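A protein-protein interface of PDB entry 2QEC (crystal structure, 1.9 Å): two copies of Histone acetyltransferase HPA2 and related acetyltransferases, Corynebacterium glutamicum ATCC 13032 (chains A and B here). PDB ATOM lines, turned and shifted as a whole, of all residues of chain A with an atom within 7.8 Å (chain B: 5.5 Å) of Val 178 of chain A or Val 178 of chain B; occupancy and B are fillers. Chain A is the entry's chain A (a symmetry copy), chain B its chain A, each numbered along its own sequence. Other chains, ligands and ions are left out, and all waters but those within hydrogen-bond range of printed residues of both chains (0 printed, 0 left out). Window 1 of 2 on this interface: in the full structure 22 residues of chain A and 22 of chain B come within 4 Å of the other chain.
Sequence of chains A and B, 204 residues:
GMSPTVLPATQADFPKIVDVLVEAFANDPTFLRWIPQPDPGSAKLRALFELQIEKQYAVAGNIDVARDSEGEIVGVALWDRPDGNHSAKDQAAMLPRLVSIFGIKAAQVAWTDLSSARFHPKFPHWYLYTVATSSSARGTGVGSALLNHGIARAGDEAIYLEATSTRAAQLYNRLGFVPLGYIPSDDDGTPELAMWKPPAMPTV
The backbone carbonyl oxygen of Pro 179 of chain B is in hydrogen-bond range of the indole nitrogen of Trp 196 of chain A, 3.1 Å away. O of Pro 179 of chain A lies within hydrogen-bond range of NE1 of Trp 196 of chain B (3.1 Å).
N of Val 178 of chain B is in hydrogen-bond range of O of Trp 196 of chain B. The backbone NH (N) of Leu 180 of chain B sits at hydrogen-bond distance from the backbone carbonyl oxygen (O) of Ala 194 of chain B (2.9 Å). The backbone NH of Val 178 of chain A lies within hydrogen-bond range of the backbone carbonyl oxygen of Trp 196 of chain A. The backbone carbonyl oxygen of Phe 177 of chain B sits at hydrogen-bond distance from the side-chain amide nitrogen of Asn 173 of chain B (2.9 Å). The backbone NH (N) of Leu 180 of chain A is in hydrogen-bond range of the backbone carbonyl oxygen (O) of Ala 194 of chain A (2.9 Å).
Among the printed residues, pairs that only touch across the chains: Val 178 of chain A with Val 178 of chain B (3.96 Å), Val 178 of chain A with Pro 198 of chain B (3.7 Å), Pro 179 of chain A with Pro 198 of chain B (3.4 Å), Leu 180 of chain A with Trp 196 of chain B (3.4 Å), Trp 196 of chain A with Leu 180 of chain B (3.4 Å), Pro 198 of chain A with Val 178 of chain B (3.7 Å), Pro 198 of chain A with Pro 179 of chain B (3.4 Å), Pro 199 of chain A with Pro 179 of chain B (3.3 Å), Pro 199 of chain A with Leu 180 of chain B (3.9 Å), Met 201 of chain A with Asn 173 of chain B (3.6 Å), Met 201 of chain A with Pro 179 of chain B (3.8 Å) and Met 201 of chain A with Met 195 of chain B (3.9 Å).
Val 178 of chain A touches two residues of chain B. Of the printed residues of chain B, Met 201 of chain A touches Asn 173 (3.6 Å), Pro 179 (3.8 Å) and Met 195 (3.9 Å). Val 178 of chain B touches just these residues of chain A: Val 178 and Pro 198. Of chain A, only Trp 196 (3.1 Å), Pro 198 (3.4 Å), Pro 199 (3.3 Å) and Met 201 (3.8 Å) come within 4 Å of Pro 179 of chain B. Printed residues of chain A within 4 Å of Met 195 of chain B: Met 201 (3.9 Å). The nearest printed residue of chain A that does not touch Asn 173 of chain B is Pro 198 of chain A (7.1 Å).
Of the 11 printed residues of chain B, 7 touch a printed residue of chain A. Printed residues of chain B that touch a printed residue of chain A: Asn 173, Val 178, Pro 179, Leu 180, Met 195, Trp 196 and Pro 198. Hydrophobic or aromatic side chains of chain B that line the printed part of chain A: Val 178, Pro 179, Leu 180, Met 195, Trp 196 and Pro 198. Printed residues of chain A that touch a printed residue of chain B: Val 178, Pro 179, Leu 180, Trp 196, Pro 198, Pro 199 and Met 201. Along chain A the printed residues that touch a printed residue of chain B span positions 178 to 201. Among the printed residues, no Asp or Glu carboxylate lies within 4 Å of a Lys or Arg side-chain nitrogen of the other chain.
Val 178 of chain B touches its own counterpart, Val 178 of chain A. Val 178 of chain A touches Pro 198 of chain B, and with the chains exchanged Pro 198 of chain A touches Val 178 of chain B. Pro 179 of chain A touches Pro 198 of chain B, and with the chains exchanged Pro 198 of chain A touches Pro 179 of chain B. Leu 180 of chain A touches Trp 196 of chain B, and with the chains exchanged Trp 196 of chain A touches Leu 180 of chain B. 11 positions are printed for both chains.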
ATOM      1  N   ILE A 159     -26.641  15.176   8.811  1.00  0.00           N
ATOM      2  CA  ILE A 159     -27.438  14.349   7.934  1.00  0.00           C
ATOM      3  C   ILE A 159     -26.527  13.764   6.823  1.00  0.00           C
ATOM      4  O   ILE A 159     -25.760  14.486   6.210  1.00  0.00           O
ATOM      5  CB  ILE A 159     -28.544  15.159   7.275  1.00  0.00           C
ATOM      6  CG1 ILE A 159     -29.298  15.997   8.317  1.00  0.00           C
ATOM      7  CG2 ILE A 159     -29.515  14.202   6.534  1.00  0.00           C
ATOM      8  CD1 ILE A 159     -30.486  16.839   7.728  1.00  0.00           C
ATOM      9  N   LEU A 161     -26.898  11.461   3.118  1.00  0.00           N
ATOM     10  CA  LEU A 161     -27.696  10.911   2.075  1.00  0.00           C
ATOM     11  C   LEU A 161     -26.805  10.527   0.889  1.00  0.00           C
ATOM     12  O   LEU A 161     -25.624  10.841   0.826  1.00  0.00           O
ATOM     13  CB  LEU A 161     -28.815  11.893   1.645  1.00  0.00           C
ATOM     14  CG  LEU A 161     -28.400  13.289   1.144  1.00  0.00           C
ATOM     15  CD1 LEU A 161     -27.881  13.254  -0.301  1.00  0.00           C
ATOM     16  CD2 LEU A 161     -29.559  14.222   1.224  1.00  0.00           C
ATOM     17  N   ALA A 169     -28.090  16.254  -6.393  1.00  0.00           N
ATOM     18  CA  ALA A 169     -26.922  16.696  -5.656  1.00  0.00           C
ATOM     19  C   ALA A 169     -26.875  18.219  -5.519  1.00  0.00           C
ATOM     20  O   ALA A 169     -26.497  18.746  -4.476  1.00  0.00           O
ATOM     21  CB  ALA A 169     -25.665  16.186  -6.348  1.00  0.00           C
ATOM     22  N   TYR A 172     -29.566  19.384  -3.014  1.00  0.00           N
ATOM     23  CA  TYR A 172     -29.074  19.121  -1.664  1.00  0.00           C
ATOM     24  C   TYR A 172     -27.929  20.039  -1.247  1.00  0.00           C
ATOM     25  O   TYR A 172     -27.908  20.494  -0.110  1.00  0.00           O
ATOM     26  CB  TYR A 172     -28.681  17.650  -1.512  1.00  0.00           C
ATOM     27  CG  TYR A 172     -29.822  16.683  -1.727  1.00  0.00           C
ATOM     28  CD1 TYR A 172     -31.033  16.884  -1.109  1.00  0.00           C
ATOM     29  CD2 TYR A 172     -29.675  15.552  -2.544  1.00  0.00           C
ATOM     30  CE1 TYR A 172     -32.082  16.003  -1.297  1.00  0.00           C
ATOM     31  CE2 TYR A 172     -30.753  14.663  -2.762  1.00  0.00           C
ATOM     32  CZ  TYR A 172     -31.945  14.896  -2.119  1.00  0.00           C
ATOM     33  OH  TYR A 172     -33.029  14.022  -2.257  1.00  0.00           O
ATOM     34  N   ASN A 173     -26.995  20.323  -2.151  1.00  0.00           N
ATOM     35  CA  ASN A 173     -25.962  21.327  -1.921  1.00  0.00           C
ATOM     36  C   ASN A 173     -26.527  22.708  -1.568  1.00  0.00           C
ATOM     37  O   ASN A 173     -25.992  23.393  -0.716  1.00  0.00           O
ATOM     38  CB  ASN A 173     -25.036  21.410  -3.142  1.00  0.00           C
ATOM     39  CG  ASN A 173     -23.793  22.249  -2.909  1.00  0.00           C
ATOM     40  OD1 ASN A 173     -23.511  23.127  -3.698  1.00  0.00           O
ATOM     41  ND2 ASN A 173     -23.001  21.937  -1.883  1.00  0.00           N
ATOM     42  N   ARG A 174     -27.602  23.126  -2.220  1.00  0.00           N
ATOM     43  CA  ARG A 174     -28.237  24.408  -1.878  1.00  0.00           C
ATOM     44  C   ARG A 174     -28.904  24.392  -0.478  1.00  0.00           C
ATOM     45  O   ARG A 174     -29.092  25.441   0.133  1.00  0.00           O
ATOM     46  CB  ARG A 174     -29.234  24.812  -2.967  1.00  0.00           C
ATOM     47  CG  ARG A 174     -28.531  25.321  -4.259  1.00  0.00           C
ATOM     48  CD  ARG A 174     -29.500  25.970  -5.217  1.00  0.00           C
ATOM     49  NE  ARG A 174     -30.548  25.039  -5.639  1.00  0.00           N
ATOM     50  CZ  ARG A 174     -30.445  24.168  -6.649  1.00  0.00           C
ATOM     51  NH1 ARG A 174     -29.323  24.076  -7.371  1.00  0.00           N
ATOM     52  NH2 ARG A 174     -31.477  23.377  -6.936  1.00  0.00           N
ATOM     53  N   LEU A 175     -29.243  23.201   0.022  1.00  0.00           N
ATOM     54  CA  LEU A 175     -29.787  23.035   1.375  1.00  0.00           C
ATOM     55  C   LEU A 175     -28.738  22.801   2.445  1.00  0.00           C
ATOM     56  O   LEU A 175     -29.089  22.515   3.593  1.00  0.00           O
ATOM     57  CB  LEU A 175     -30.787  21.870   1.381  1.00  0.00           C
ATOM     58  CG  LEU A 175     -31.975  22.072   0.467  1.00  0.00           C
ATOM     59  CD1 LEU A 175     -32.705  20.748   0.261  1.00  0.00           C
ATOM     60  CD2 LEU A 175     -32.907  23.108   1.057  1.00  0.00           C
ATOM     61  N   GLY A 176     -27.466  22.966   2.092  1.00  0.00           N
ATOM     62  CA  GLY A 176     -26.366  22.841   3.043  1.00  0.00           C
ATOM     63  C   GLY A 176     -25.611  21.523   3.082  1.00  0.00           C
ATOM     64  O   GLY A 176     -24.744  21.365   3.922  1.00  0.00           O
ATOM     65  N   PHE A 177     -25.928  20.568   2.209  1.00  0.00           N
ATOM     66  CA  PHE A 177     -25.106  19.343   2.072  1.00  0.00           C
ATOM     67  C   PHE A 177     -23.828  19.577   1.276  1.00  0.00           C
ATOM     68  O   PHE A 177     -23.846  20.197   0.216  1.00  0.00           O
ATOM     69  CB  PHE A 177     -25.903  18.230   1.397  1.00  0.00           C
ATOM     70  CG  PHE A 177     -27.030  17.693   2.228  1.00  0.00           C
ATOM     71  CD1 PHE A 177     -28.230  18.398   2.348  1.00  0.00           C
ATOM     72  CD2 PHE A 177     -26.889  16.504   2.910  1.00  0.00           C
ATOM     73  CE1 PHE A 177     -29.262  17.909   3.114  1.00  0.00           C
ATOM     74  CE2 PHE A 177     -27.911  15.986   3.650  1.00  0.00           C
ATOM     75  CZ  PHE A 177     -29.119  16.711   3.765  1.00  0.00           C
ATOM     76  N   VAL A 178     -22.703  19.061   1.768  1.00  0.00           N
ATOM     77  CA  VAL A 178     -21.450  19.106   1.003  1.00  0.00           C
ATOM     78  C   VAL A 178     -21.135  17.699   0.456  1.00  0.00           C
ATOM     79  O   VAL A 178     -21.580  16.701   1.033  1.00  0.00           O
ATOM     80  CB  VAL A 178     -20.242  19.610   1.834  1.00  0.00           C
ATOM     81  CG1 VAL A 178     -20.478  21.013   2.356  1.00  0.00           C
ATOM     82  CG2 VAL A 178     -19.900  18.658   2.933  1.00  0.00           C
ATOM     83  N   PRO A 179     -20.417  17.610  -0.700  1.00  0.00           N
ATOM     84  CA  PRO A 179     -20.125  16.258  -1.177  1.00  0.00           C
ATOM     85  C   PRO A 179     -19.075  15.536  -0.317  1.00  0.00           C
ATOM     86  O   PRO A 179     -18.138  16.152   0.162  1.00  0.00           O
ATOM     87  CB  PRO A 179     -19.556  16.480  -2.597  1.00  0.00           C
ATOM     88  CG  PRO A 179     -19.086  17.921  -2.628  1.00  0.00           C
ATOM     89  CD  PRO A 179     -19.974  18.660  -1.651  1.00  0.00           C
ATOM     90  N   LEU A 180     -19.246  14.224  -0.181  1.00  0.00           N
ATOM     91  CA  LEU A 180     -18.218  13.337   0.349  1.00  0.00           C
ATOM     92  C   LEU A 180     -17.507  12.665  -0.841  1.00  0.00           C
ATOM     93  O   LEU A 180     -16.310  12.765  -0.988  1.00  0.00           O
ATOM     94  CB  LEU A 180     -18.866  12.305   1.261  1.00  0.00           C
ATOM     95  CG  LEU A 180     -19.452  12.812   2.590  1.00  0.00           C
ATOM     96  CD1 LEU A 180     -20.217  11.680   3.294  1.00  0.00           C
ATOM     97  CD2 LEU A 180     -18.338  13.255   3.527  1.00  0.00           C
ATOM     98  N   GLY A 181     -18.259  12.029  -1.715  1.00  0.00           N
ATOM     99  CA  GLY A 181     -17.686  11.465  -2.949  1.00  0.00           C
ATOM    100  C   GLY A 181     -18.614  10.420  -3.523  1.00  0.00           C
ATOM    101  O   GLY A 181     -19.704  10.208  -2.996  1.00  0.00           O
ATOM    102  N   LEU A 193     -23.731   9.896  -5.317  1.00  0.00           N
ATOM    103  CA  LEU A 193     -22.873  10.886  -4.668  1.00  0.00           C
ATOM    104  C   LEU A 193     -23.287  10.991  -3.187  1.00  0.00           C
ATOM    105  O   LEU A 193     -24.335  11.521  -2.863  1.00  0.00           O
ATOM    106  CB  LEU A 193     -23.007  12.251  -5.350  1.00  0.00           C
ATOM    107  CG  LEU A 193     -22.090  13.350  -4.741  1.00  0.00           C
ATOM    108  CD1 LEU A 193     -20.662  12.949  -4.714  1.00  0.00           C
ATOM    109  CD2 LEU A 193     -22.232  14.667  -5.433  1.00  0.00           C
ATOM    110  N   ALA A 194     -22.463  10.432  -2.302  1.00  0.00           N
ATOM    111  CA  ALA A 194     -22.646  10.565  -0.862  1.00  0.00           C
ATOM    112  C   ALA A 194     -22.479  12.017  -0.502  1.00  0.00           C
ATOM    113  O   ALA A 194     -21.515  12.662  -0.952  1.00  0.00           O
ATOM    114  CB  ALA A 194     -21.551   9.747  -0.128  1.00  0.00           C
ATOM    115  N   MET A 195     -23.343  12.521   0.376  1.00  0.00           N
ATOM    116  CA  MET A 195     -23.278  13.909   0.827  1.00  0.00           C
ATOM    117  C   MET A 195     -23.538  14.003   2.330  1.00  0.00           C
ATOM    118  O   MET A 195     -24.110  13.111   2.919  1.00  0.00           O
ATOM    119  CB  MET A 195     -24.322  14.756   0.081  1.00  0.00           C
ATOM    120  CG  MET A 195     -24.253  14.599  -1.424  1.00  0.00           C
ATOM    121  SD  MET A 195     -25.308  15.851  -2.399  1.00  0.00           S
ATOM    122  CE  MET A 195     -24.022  17.064  -2.337  1.00  0.00           C
ATOM    123  N   TRP A 196     -23.102  15.126   2.914  1.00  0.00           N
ATOM    124  CA  TRP A 196     -23.134  15.370   4.331  1.00  0.00           C
ATOM    125  C   TRP A 196     -23.603  16.778   4.602  1.00  0.00           C
ATOM    126  O   TRP A 196     -22.930  17.739   4.180  1.00  0.00           O
ATOM    127  CB  TRP A 196     -21.694  15.252   4.834  1.00  0.00           C
ATOM    128  CG  TRP A 196     -21.427  15.332   6.318  1.00  0.00           C
ATOM    129  CD1 TRP A 196     -20.782  16.331   6.974  1.00  0.00           C
ATOM    130  CD2 TRP A 196     -21.716  14.333   7.294  1.00  0.00           C
ATOM    131  NE1 TRP A 196     -20.665  16.025   8.307  1.00  0.00           N
ATOM    132  CE2 TRP A 196     -21.232  14.804   8.533  1.00  0.00           C
ATOM    133  CE3 TRP A 196     -22.343  13.084   7.245  1.00  0.00           C
ATOM    134  CZ2 TRP A 196     -21.350  14.067   9.706  1.00  0.00           C
ATOM    135  CZ3 TRP A 196     -22.471  12.352   8.420  1.00  0.00           C
ATOM    136  CH2 TRP A 196     -21.971  12.838   9.628  1.00  0.00           C
ATOM    137  N   LYS A 197     -24.664  16.916   5.388  1.00  0.00           N
ATOM    138  CA  LYS A 197     -24.986  18.212   6.003  1.00  0.00           C
ATOM    139  C   LYS A 197     -24.367  18.235   7.398  1.00  0.00           C
ATOM    140  O   LYS A 197     -24.727  17.434   8.260  1.00  0.00           O
ATOM    141  CB  LYS A 197     -26.488  18.465   6.047  1.00  0.00           C
ATOM    142  CG  LYS A 197     -26.830  19.786   6.701  1.00  0.00           C
ATOM    143  CD  LYS A 197     -28.194  20.272   6.361  1.00  0.00           C
ATOM    144  CE  LYS A 197     -28.471  21.672   6.910  1.00  0.00           C
ATOM    145  NZ  LYS A 197     -28.082  21.899   8.352  1.00  0.00           N
ATOM    146  N   PRO A 198     -23.375  19.130   7.613  1.00  0.00           N
ATOM    147  CA  PRO A 198     -22.613  19.020   8.835  1.00  0.00           C
ATOM    148  C   PRO A 198     -23.374  19.414  10.087  1.00  0.00           C
ATOM    149  O   PRO A 198     -24.369  20.145   9.995  1.00  0.00           O
ATOM    150  CB  PRO A 198     -21.413  19.938   8.617  1.00  0.00           C
ATOM    151  CG  PRO A 198     -21.778  20.838   7.503  1.00  0.00           C
ATOM    152  CD  PRO A 198     -22.941  20.237   6.742  1.00  0.00           C
ATOM    153  N   PRO A 199     -22.897  18.944  11.239  1.00  0.00           N
ATOM    154  CA  PRO A 199     -23.469  19.387  12.489  1.00  0.00           C
ATOM    155  C   PRO A 199     -23.012  20.809  12.752  1.00  0.00           C
ATOM    156  O   PRO A 199     -22.109  21.298  12.083  1.00  0.00           O
ATOM    157  CB  PRO A 199     -22.916  18.386  13.491  1.00  0.00           C
ATOM    158  CG  PRO A 199     -21.579  18.022  12.947  1.00  0.00           C
ATOM    159  CD  PRO A 199     -21.804  17.984  11.447  1.00  0.00           C
ATOM    160  N   MET A 201     -21.080  23.798  14.339  1.00  0.00           N
ATOM    161  CA  MET A 201     -19.752  23.973  14.892  1.00  0.00           C
ATOM    162  C   MET A 201     -19.882  24.181  16.390  1.00  0.00           C
ATOM    163  O   MET A 201     -20.927  24.627  16.844  1.00  0.00           O
ATOM    164  CB  MET A 201     -19.076  25.169  14.224  1.00  0.00           C
ATOM    165  CG  MET A 201     -18.498  24.846  12.814  1.00  0.00           C
ATOM    166  SD  MET A 201     -16.899  23.965  12.991  1.00  0.00           S
ATOM    167  CE  MET A 201     -15.771  25.316  13.750  1.00  0.00           C
ATOM    168  N   ASN B 173     -12.436  25.680   9.767  1.00  0.00           N
ATOM    169  CA  ASN B 173     -13.748  26.060   9.256  1.00  0.00           C
ATOM    170  C   ASN B 173     -13.713  27.310   8.367  1.00  0.00           C
ATOM    171  O   ASN B 173     -14.398  27.371   7.364  1.00  0.00           O
ATOM    172  CB  ASN B 173     -14.728  26.244  10.421  1.00  0.00           C
ATOM    173  CG  ASN B 173     -16.172  26.406   9.985  1.00  0.00           C
ATOM    174  OD1 ASN B 173     -16.820  27.342  10.405  1.00  0.00           O
ATOM    175  ND2 ASN B 173     -16.711  25.460   9.215  1.00  0.00           N
ATOM    176  N   GLY B 176     -12.663  26.504   4.819  1.00  0.00           N
ATOM    177  CA  GLY B 176     -13.563  25.629   4.071  1.00  0.00           C
ATOM    178  C   GLY B 176     -13.766  24.215   4.587  1.00  0.00           C
ATOM    179  O   GLY B 176     -14.446  23.443   3.937  1.00  0.00           O
ATOM    180  N   PHE B 177     -13.184  23.851   5.728  1.00  0.00           N
ATOM    181  CA  PHE B 177     -13.499  22.557   6.378  1.00  0.00           C
ATOM    182  C   PHE B 177     -14.828  22.579   7.122  1.00  0.00           C
ATOM    183  O   PHE B 177     -15.122  23.510   7.867  1.00  0.00           O
ATOM    184  CB  PHE B 177     -12.397  22.163   7.359  1.00  0.00           C
ATOM    185  CG  PHE B 177     -11.093  21.815   6.708  1.00  0.00           C
ATOM    186  CD1 PHE B 177     -10.236  22.815   6.241  1.00  0.00           C
ATOM    187  CD2 PHE B 177     -10.728  20.497   6.536  1.00  0.00           C
ATOM    188  CE1 PHE B 177      -9.041  22.497   5.640  1.00  0.00           C
ATOM    189  CE2 PHE B 177      -9.534  20.161   5.969  1.00  0.00           C
ATOM    190  CZ  PHE B 177      -8.678  21.182   5.499  1.00  0.00           C
ATOM    191  N   VAL B 178     -15.639  21.537   6.946  1.00  0.00           N
ATOM    192  CA  VAL B 178     -16.872  21.396   7.730  1.00  0.00           C
ATOM    193  C   VAL B 178     -16.681  20.290   8.789  1.00  0.00           C
ATOM    194  O   VAL B 178     -15.854  19.392   8.597  1.00  0.00           O
ATOM    195  CB  VAL B 178     -18.114  21.062   6.866  1.00  0.00           C
ATOM    196  CG1 VAL B 178     -18.380  22.144   5.838  1.00  0.00           C
ATOM    197  CG2 VAL B 178     -17.994  19.713   6.234  1.00  0.00           C
ATOM    198  N   PRO B 179     -17.400  20.381   9.945  1.00  0.00           N
ATOM    199  CA  PRO B 179     -17.202  19.305  10.915  1.00  0.00           C
ATOM    200  C   PRO B 179     -17.839  17.978  10.471  1.00  0.00           C
ATOM    201  O   PRO B 179     -18.899  17.972   9.868  1.00  0.00           O
ATOM    202  CB  PRO B 179     -17.919  19.815  12.185  1.00  0.00           C
ATOM    203  CG  PRO B 179     -18.892  20.874  11.708  1.00  0.00           C
ATOM    204  CD  PRO B 179     -18.273  21.465  10.461  1.00  0.00           C
ATOM    205  N   LEU B 180     -17.183  16.877  10.826  1.00  0.00           N
ATOM    206  CA  LEU B 180     -17.762  15.542  10.747  1.00  0.00           C
ATOM    207  C   LEU B 180     -18.260  15.155  12.153  1.00  0.00           C
ATOM    208  O   LEU B 180     -19.415  14.849  12.342  1.00  0.00           O
ATOM    209  CB  LEU B 180     -16.709  14.566  10.243  1.00  0.00           C
ATOM    210  CG  LEU B 180     -16.256  14.715   8.781  1.00  0.00           C
ATOM    211  CD1 LEU B 180     -15.073  13.774   8.498  1.00  0.00           C
ATOM    212  CD2 LEU B 180     -17.381  14.324   7.834  1.00  0.00           C
ATOM    213  N   ALA B 194     -12.955  15.655  13.966  1.00  0.00           N
ATOM    214  CA  ALA B 194     -12.726  15.295  12.572  1.00  0.00           C
ATOM    215  C   ALA B 194     -13.394  16.329  11.706  1.00  0.00           C
ATOM    216  O   ALA B 194     -14.560  16.686  11.953  1.00  0.00           O
ATOM    217  CB  ALA B 194     -13.379  13.917  12.285  1.00  0.00           C
ATOM    218  N   MET B 195     -12.716  16.749  10.641  1.00  0.00           N
ATOM    219  CA  MET B 195     -13.259  17.733   9.708  1.00  0.00           C
ATOM    220  C   MET B 195     -12.940  17.345   8.264  1.00  0.00           C
ATOM    221  O   MET B 195     -12.034  16.579   8.012  1.00  0.00           O
ATOM    222  CB  MET B 195     -12.665  19.120   9.999  1.00  0.00           C
ATOM    223  CG  MET B 195     -12.784  19.527  11.453  1.00  0.00           C
ATOM    224  SD  MET B 195     -12.350  21.349  11.803  1.00  0.00           S
ATOM    225  CE  MET B 195     -13.986  21.876  11.388  1.00  0.00           C
ATOM    226  N   TRP B 196     -13.717  17.916   7.337  1.00  0.00           N
ATOM    227  CA  TRP B 196     -13.671  17.603   5.933  1.00  0.00           C
ATOM    228  C   TRP B 196     -13.742  18.870   5.118  1.00  0.00           C
ATOM    229  O   TRP B 196     -14.754  19.594   5.198  1.00  0.00           O
ATOM    230  CB  TRP B 196     -14.922  16.777   5.623  1.00  0.00           C
ATOM    231  CG  TRP B 196     -15.086  16.188   4.242  1.00  0.00           C
ATOM    232  CD1 TRP B 196     -16.004  16.549   3.309  1.00  0.00           C
ATOM    233  CD2 TRP B 196     -14.372  15.081   3.694  1.00  0.00           C
ATOM    234  NE1 TRP B 196     -15.898  15.745   2.202  1.00  0.00           N
ATOM    235  CE2 TRP B 196     -14.901  14.835   2.409  1.00  0.00           C
ATOM    236  CE3 TRP B 196     -13.331  14.274   4.161  1.00  0.00           C
ATOM    237  CZ2 TRP B 196     -14.429  13.812   1.593  1.00  0.00           C
ATOM    238  CZ3 TRP B 196     -12.851  13.258   3.341  1.00  0.00           C
ATOM    239  CH2 TRP B 196     -13.403  13.030   2.080  1.00  0.00           C
ATOM    240  N   LYS B 197     -12.752  19.087   4.261  1.00  0.00           N
ATOM    241  CA  LYS B 197     -12.890  20.075   3.181  1.00  0.00           C
ATOM    242  C   LYS B 197     -13.365  19.341   1.931  1.00  0.00           C
ATOM    243  O   LYS B 197     -12.669  18.471   1.408  1.00  0.00           O
ATOM    244  CB  LYS B 197     -11.592  20.833   2.932  1.00  0.00           C
ATOM    245  CG  LYS B 197     -11.718  21.836   1.805  1.00  0.00           C
ATOM    246  CD  LYS B 197     -10.663  22.884   1.833  1.00  0.00           C
ATOM    247  CE  LYS B 197     -10.887  23.969   0.779  1.00  0.00           C
ATOM    248  NZ  LYS B 197     -11.222  23.475  -0.609  1.00  0.00           N
ATOM    249  N   PRO B 198     -14.600  19.650   1.471  1.00  0.00           N
ATOM    250  CA  PRO B 198     -15.172  18.813   0.442  1.00  0.00           C
ATOM    251  C   PRO B 198     -14.520  18.961  -0.921  1.00  0.00           C
ATOM    252  O   PRO B 198     -13.879  19.986  -1.186  1.00  0.00           O
ATOM    253  CB  PRO B 198     -16.640  19.227   0.388  1.00  0.00           C
ATOM    254  CG  PRO B 198     -16.722  20.545   1.052  1.00  0.00           C
ATOM    255  CD  PRO B 198     -15.480  20.755   1.892  1.00  0.00           C
